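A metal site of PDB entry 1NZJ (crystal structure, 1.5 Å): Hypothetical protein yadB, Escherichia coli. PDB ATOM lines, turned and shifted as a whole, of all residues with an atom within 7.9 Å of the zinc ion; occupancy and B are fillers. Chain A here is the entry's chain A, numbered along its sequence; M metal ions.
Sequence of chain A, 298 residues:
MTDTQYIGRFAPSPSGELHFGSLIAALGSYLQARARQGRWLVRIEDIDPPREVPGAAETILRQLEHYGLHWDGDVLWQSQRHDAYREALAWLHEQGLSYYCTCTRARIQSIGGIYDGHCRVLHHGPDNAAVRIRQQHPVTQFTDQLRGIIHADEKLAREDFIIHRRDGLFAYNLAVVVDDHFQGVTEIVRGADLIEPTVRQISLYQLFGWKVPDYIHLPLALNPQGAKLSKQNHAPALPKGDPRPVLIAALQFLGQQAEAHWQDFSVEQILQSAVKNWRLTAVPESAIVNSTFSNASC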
ATOM      1  N   TYR A  99      -7.385 -21.854  25.363  1.00  0.00           N
ATOM      2  CA  TYR A  99      -5.996 -22.185  25.586  1.00  0.00           C
ATOM      3  C   TYR A  99      -5.359 -21.267  26.633  1.00  0.00           C
ATOM      4  O   TYR A  99      -5.919 -20.218  26.975  1.00  0.00           O
ATOM      5  CB  TYR A  99      -5.182 -22.124  24.287  1.00  0.00           C
ATOM      6  CG  TYR A  99      -5.221 -20.807  23.530  1.00  0.00           C
ATOM      7  CD1 TYR A  99      -4.261 -19.837  23.747  1.00  0.00           C
ATOM      8  CD2 TYR A  99      -6.235 -20.526  22.604  1.00  0.00           C
ATOM      9  CE1 TYR A  99      -4.273 -18.634  23.051  1.00  0.00           C
ATOM     10  CE2 TYR A  99      -6.274 -19.314  21.922  1.00  0.00           C
ATOM     11  CZ  TYR A  99      -5.272 -18.377  22.127  1.00  0.00           C
ATOM     12  OH  TYR A  99      -5.237 -17.201  21.437  1.00  0.00           O
ATOM     13  N   TYR A 100      -4.218 -21.694  27.164  1.00  0.00           N
ATOM     14  CA  TYR A 100      -3.482 -20.966  28.189  1.00  0.00           C
ATOM     15  C   TYR A 100      -2.433 -20.047  27.558  1.00  0.00           C
ATOM     16  O   TYR A 100      -1.635 -20.470  26.718  1.00  0.00           O
ATOM     17  CB  TYR A 100      -2.855 -21.943  29.200  1.00  0.00           C
ATOM     18  CG  TYR A 100      -3.874 -22.793  29.913  1.00  0.00           C
ATOM     19  CD1 TYR A 100      -3.968 -24.159  29.683  1.00  0.00           C
ATOM     20  CD2 TYR A 100      -4.778 -22.224  30.797  1.00  0.00           C
ATOM     21  CE1 TYR A 100      -4.913 -24.947  30.324  1.00  0.00           C
ATOM     22  CE2 TYR A 100      -5.742 -23.015  31.453  1.00  0.00           C
ATOM     23  CZ  TYR A 100      -5.805 -24.370  31.204  1.00  0.00           C
ATOM     24  OH  TYR A 100      -6.752 -25.160  31.835  1.00  0.00           O
ATOM     25  N   CYS A 101      -2.445 -18.775  27.958  1.00  0.00           N
ATOM     26  CA  CYS A 101      -1.542 -17.751  27.432  1.00  0.00           C
ATOM     27  C   CYS A 101      -0.592 -17.233  28.518  1.00  0.00           C
ATOM     28  O   CYS A 101      -1.028 -16.761  29.581  1.00  0.00           O
ATOM     29  CB  CYS A 101      -2.362 -16.592  26.864  1.00  0.00           C
ATOM     30  SG  CYS A 101      -1.396 -15.113  26.473  1.00  0.00           S
ATOM     31  N   THR A 102       0.707 -17.293  28.239  1.00  0.00           N
ATOM     32  CA  THR A 102       1.721 -16.860  29.205  1.00  0.00           C
ATOM     33  C   THR A 102       2.350 -15.525  28.796  1.00  0.00           C
ATOM     34  O   THR A 102       3.376 -15.130  29.348  1.00  0.00           O
ATOM     35  CB  THR A 102       2.833 -17.929  29.309  1.00  0.00           C
ATOM     36  OG1 THR A 102       3.342 -18.213  28.009  1.00  0.00           O
ATOM     37  CG2 THR A 102       2.267 -19.259  29.776  1.00  0.00           C
ATOM     38  N   CYS A 103       1.727 -14.824  27.857  1.00  0.00           N
ATOM     39  CA  CYS A 103       2.281 -13.553  27.395  1.00  0.00           C
ATOM     40  C   CYS A 103       2.166 -12.477  28.461  1.00  0.00           C
ATOM     41  O   CYS A 103       1.173 -12.417  29.185  1.00  0.00           O
ATOM     42  CB  CYS A 103       1.594 -13.084  26.092  1.00  0.00           C
ATOM     43  SG  CYS A 103       1.863 -14.198  24.706  1.00  0.00           S
ATOM     44  N   THR A 104       3.163 -11.595  28.532  1.00  0.00           N
ATOM     45  CA  THR A 104       3.136 -10.509  29.491  1.00  0.00           C
ATOM     46  C   THR A 104       2.277  -9.353  29.007  1.00  0.00           C
ATOM     47  O   THR A 104       2.020  -9.193  27.812  1.00  0.00           O
ATOM     48  CB  THR A 104       4.544  -9.957  29.775  1.00  0.00           C
ATOM     49  OG1 THR A 104       5.129  -9.455  28.566  1.00  0.00           O
ATOM     50  CG2 THR A 104       5.488 -11.055  30.259  1.00  0.00           C
ATOM     51  N   ARG A 107       4.322  -7.357  26.474  1.00  0.00           N
ATOM     52  CA  ARG A 107       4.310  -7.881  25.115  1.00  0.00           C
ATOM     53  C   ARG A 107       3.054  -7.418  24.360  1.00  0.00           C
ATOM     54  O   ARG A 107       3.149  -6.892  23.235  1.00  0.00           O
ATOM     55  CB  ARG A 107       4.384  -9.409  25.093  1.00  0.00           C
ATOM     56  CG  ARG A 107       4.290  -9.999  23.704  1.00  0.00           C
ATOM     57  CD  ARG A 107       4.300 -11.532  23.625  1.00  0.00           C
ATOM     58  NE  ARG A 107       4.333 -11.857  22.211  1.00  0.00           N
ATOM     59  CZ  ARG A 107       3.267 -12.013  21.426  1.00  0.00           C
ATOM     60  NH1 ARG A 107       2.042 -12.076  21.926  1.00  0.00           N
ATOM     61  NH2 ARG A 107       3.445 -12.197  20.126  1.00  0.00           N
ATOM     62  N   ILE A 108       1.892  -7.576  24.982  1.00  0.00           N
ATOM     63  CA  ILE A 108       0.621  -7.218  24.339  1.00  0.00           C
ATOM     64  C   ILE A 108       0.578  -5.697  24.071  1.00  0.00           C
ATOM     65  O   ILE A 108       0.165  -5.257  22.996  1.00  0.00           O
ATOM     66  CB  ILE A 108      -0.622  -7.673  25.171  1.00  0.00           C
ATOM     67  CG1 ILE A 108      -0.664  -9.200  25.438  1.00  0.00           C
ATOM     68  CG2 ILE A 108      -1.910  -7.200  24.516  1.00  0.00           C
ATOM     69  CD1 ILE A 108       0.116 -10.077  24.535  1.00  0.00           C
ATOM     70  N   TYR A 115      -4.442  -8.824  21.200  1.00  0.00           N
ATOM     71  CA  TYR A 115      -3.694 -10.076  21.123  1.00  0.00           C
ATOM     72  C   TYR A 115      -3.641 -10.644  19.717  1.00  0.00           C
ATOM     73  O   TYR A 115      -4.597 -10.502  18.945  1.00  0.00           O
ATOM     74  CB  TYR A 115      -4.324 -11.091  22.069  1.00  0.00           C
ATOM     75  CG  TYR A 115      -3.479 -12.306  22.318  1.00  0.00           C
ATOM     76  CD1 TYR A 115      -2.203 -12.194  22.876  1.00  0.00           C
ATOM     77  CD2 TYR A 115      -3.947 -13.588  22.038  1.00  0.00           C
ATOM     78  CE1 TYR A 115      -1.419 -13.314  23.129  1.00  0.00           C
ATOM     79  CE2 TYR A 115      -3.160 -14.716  22.260  1.00  0.00           C
ATOM     80  CZ  TYR A 115      -1.908 -14.569  22.816  1.00  0.00           C
ATOM     81  OH  TYR A 115      -1.147 -15.669  23.090  1.00  0.00           O
ATOM     82  N   ASP A 116      -2.522 -11.301  19.402  1.00  0.00           N
ATOM     83  CA  ASP A 116      -2.254 -11.862  18.082  1.00  0.00           C
ATOM     84  C   ASP A 116      -2.434 -13.367  17.945  1.00  0.00           C
ATOM     85  O   ASP A 116      -2.164 -13.933  16.888  1.00  0.00           O
ATOM     86  CB  ASP A 116      -0.817 -11.505  17.647  1.00  0.00           C
ATOM     87  CG  ASP A 116       0.248 -12.140  18.536  1.00  0.00           C
ATOM     88  OD1 ASP A 116      -0.029 -12.494  19.716  1.00  0.00           O
ATOM     89  OD2 ASP A 116       1.429 -12.290  18.114  1.00  0.00           O
ATOM     90  N   GLY A 117      -2.881 -14.025  19.011  1.00  0.00           N
ATOM     91  CA  GLY A 117      -3.011 -15.467  19.027  1.00  0.00           C
ATOM     92  C   GLY A 117      -1.715 -16.253  19.173  1.00  0.00           C
ATOM     93  O   GLY A 117      -1.684 -17.439  18.833  1.00  0.00           O
ATOM     94  N   HIS A 118      -0.678 -15.627  19.733  1.00  0.00           N
ATOM     95  CA  HIS A 118       0.644 -16.254  19.943  1.00  0.00           C
ATOM     96  C   HIS A 118       0.582 -17.668  20.546  1.00  0.00           C
ATOM     97  O   HIS A 118       1.233 -18.590  20.028  1.00  0.00           O
ATOM     98  CB  HIS A 118       1.523 -15.343  20.843  1.00  0.00           C
ATOM     99  CG  HIS A 118       2.907 -15.857  21.087  1.00  0.00           C
ATOM    100  ND1 HIS A 118       3.220 -16.720  22.122  1.00  0.00           N
ATOM    101  CD2 HIS A 118       4.083 -15.623  20.445  1.00  0.00           C
ATOM    102  CE1 HIS A 118       4.507 -16.992  22.103  1.00  0.00           C
ATOM    103  NE2 HIS A 118       5.058 -16.336  21.098  1.00  0.00           N
ATOM    104  N   CYS A 119      -0.193 -17.847  21.621  1.00  0.00           N
ATOM    105  CA  CYS A 119      -0.204 -19.097  22.364  1.00  0.00           C
ATOM    106  C   CYS A 119      -1.215 -20.141  21.829  1.00  0.00           C
ATOM    107  O   CYS A 119      -1.327 -21.260  22.366  1.00  0.00           O
ATOM    108  CB  CYS A 119      -0.430 -18.821  23.864  1.00  0.00           C
ATOM    109  SG  CYS A 119       0.908 -17.877  24.674  1.00  0.00           S
ATOM    110  N   ARG A 120      -1.912 -19.801  20.745  1.00  0.00           N
ATOM    111  CA  ARG A 120      -3.042 -20.590  20.221  1.00  0.00           C
ATOM    112  C   ARG A 120      -2.727 -22.069  19.914  1.00  0.00           C
ATOM    113  O   ARG A 120      -3.588 -22.925  20.111  1.00  0.00           O
ATOM    114  CB  ARG A 120      -3.613 -19.884  18.975  1.00  0.00           C
ATOM    115  CG  ARG A 120      -4.888 -20.399  18.401  1.00  0.00           C
ATOM    116  CD  ARG A 120      -5.524 -19.456  17.379  1.00  0.00           C
ATOM    117  NE  ARG A 120      -6.568 -20.120  16.587  1.00  0.00           N
ATOM    118  CZ  ARG A 120      -7.877 -19.846  16.600  1.00  0.00           C
ATOM    119  NH1 ARG A 120      -8.400 -18.887  17.385  1.00  0.00           N
ATOM    120  NH2 ARG A 120      -8.691 -20.558  15.820  1.00  0.00           N
ATOM    121  N   LEU A 122       0.516 -23.466  21.028  1.00  0.00           N
ATOM    122  CA  LEU A 122       1.696 -23.789  21.821  1.00  0.00           C
ATOM    123  C   LEU A 122       1.444 -24.790  22.951  1.00  0.00           C
ATOM    124  O   LEU A 122       2.404 -25.314  23.513  1.00  0.00           O
ATOM    125  CB  LEU A 122       2.333 -22.519  22.369  1.00  0.00           C
ATOM    126  CG  LEU A 122       2.845 -21.559  21.295  1.00  0.00           C
ATOM    127  CD1 LEU A 122       3.529 -20.380  21.926  1.00  0.00           C
ATOM    128  CD2 LEU A 122       3.785 -22.257  20.305  1.00  0.00           C
ATOM    129  N   HIS A 124       0.625 -24.589  26.081  1.00  0.00           N
ATOM    130  CA  HIS A 124       1.067 -24.294  27.457  1.00  0.00           C
ATOM    131  C   HIS A 124       0.084 -24.858  28.487  1.00  0.00           C
ATOM    132  O   HIS A 124      -1.105 -24.993  28.218  1.00  0.00           O
ATOM    133  CB  HIS A 124       1.174 -22.790  27.706  1.00  0.00           C
ATOM    134  CG  HIS A 124       2.200 -22.089  26.867  1.00  0.00           C
ATOM    135  ND1 HIS A 124       3.397 -22.679  26.498  1.00  0.00           N
ATOM    136  CD2 HIS A 124       2.215 -20.847  26.334  1.00  0.00           C
ATOM    137  CE1 HIS A 124       4.094 -21.817  25.771  1.00  0.00           C
ATOM    138  NE2 HIS A 124       3.397 -20.698  25.657  1.00  0.00           N
ATOM    139  N   ALA A 130      -3.037 -16.915  31.767  1.00  0.00           N
ATOM    140  CA  ALA A 130      -4.419 -16.528  31.520  1.00  0.00           C
ATOM    141  C   ALA A 130      -5.087 -17.577  30.635  1.00  0.00           C
ATOM    142  O   ALA A 130      -4.408 -18.384  30.013  1.00  0.00           O
ATOM    143  CB  ALA A 130      -4.459 -15.137  30.840  1.00  0.00           C
ATOM    144  N   ARG A 132      -7.572 -17.831  27.338  1.00  0.00           N
ATOM    145  CA  ARG A 132      -8.192 -17.122  26.228  1.00  0.00           C
ATOM    146  C   ARG A 132      -9.134 -18.050  25.462  1.00  0.00           C
ATOM    147  O   ARG A 132      -8.902 -19.262  25.356  1.00  0.00           O
ATOM    148  CB  ARG A 132      -7.133 -16.597  25.264  1.00  0.00           C
ATOM    149  CG  ARG A 132      -6.225 -15.500  25.853  1.00  0.00           C
ATOM    150  CD  ARG A 132      -5.192 -14.976  24.863  1.00  0.00           C
ATOM    151  NE  ARG A 132      -4.423 -13.857  25.405  1.00  0.00           N
ATOM    152  CZ  ARG A 132      -4.827 -12.588  25.412  1.00  0.00           C
ATOM    153  NH1 ARG A 132      -6.003 -12.235  24.895  1.00  0.00           N
ATOM    154  NH2 ARG A 132      -4.058 -11.658  25.954  1.00  0.00           N
ATOM    155  N   ARG A 166      -4.996 -13.904  34.452  1.00  0.00           N
ATOM    156  CA  ARG A 166      -3.805 -14.491  35.049  1.00  0.00           C
ATOM    157  C   ARG A 166      -3.779 -14.307  36.565  1.00  0.00           C
ATOM    158  O   ARG A 166      -3.259 -15.154  37.278  1.00  0.00           O
ATOM    159  CB  ARG A 166      -2.554 -13.844  34.434  1.00  0.00           C
ATOM    160  CG  ARG A 166      -1.231 -14.505  34.756  1.00  0.00           C
ATOM    161  CD  ARG A 166      -0.092 -13.923  33.940  1.00  0.00           C
ATOM    162  NE  ARG A 166       1.112 -14.755  33.970  1.00  0.00           N
ATOM    163  CZ  ARG A 166       2.124 -14.657  33.102  1.00  0.00           C
ATOM    164  NH1 ARG A 166       2.085 -13.767  32.114  1.00  0.00           N
ATOM    165  NH2 ARG A 166       3.171 -15.462  33.213  1.00  0.00           N
HETATM  166 ZN    ZN M   1       0.050 -15.721  24.763  1.00  0.00          ZN
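The side-chain hydroxyl (OH) of Tyr 115 sits close to the backbone NH (N) of His 118, at 3.4 Å.
The guanidinium group (NE) of Arg 132 sits close to the side-chain sulfur (SG) of Cys 101 (3.4 Å).
The backbone NH of Thr 102 lies close to the side-chain sulfur of Cys 119.
ND1 of His 118 lies close to SG of Cys 119, 3.6 Å away.
SG of Cys 103 sits close to NH1 of Arg 107.
The backbone carbonyl oxygen of Cys 103 sits at hydrogen-bond distance from the guanidinium group of Arg 166, 3.4 Å away.
NE2 of His 124 lies close to OG1 of Thr 102 (3.4 Å).
The backbone carbonyl oxygen (O) of Thr 102 is in hydrogen-bond range of the guanidinium group (NH1) of Arg 166 (3.3 Å).
The zinc ion is bound by OH of Tyr 115 (2.1 Å), SG of Cys 101 (2.3 Å), SG of Cys 119 (2.3 Å) and SG of Cys 103 (2.4 Å).
The zinc ion has four donor atoms within binding distance.
N of Thr 102 touches the zinc ion, at 3.9 Å.
Of the 19 residues printed, 5 come within 4 Å of the zinc ion.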
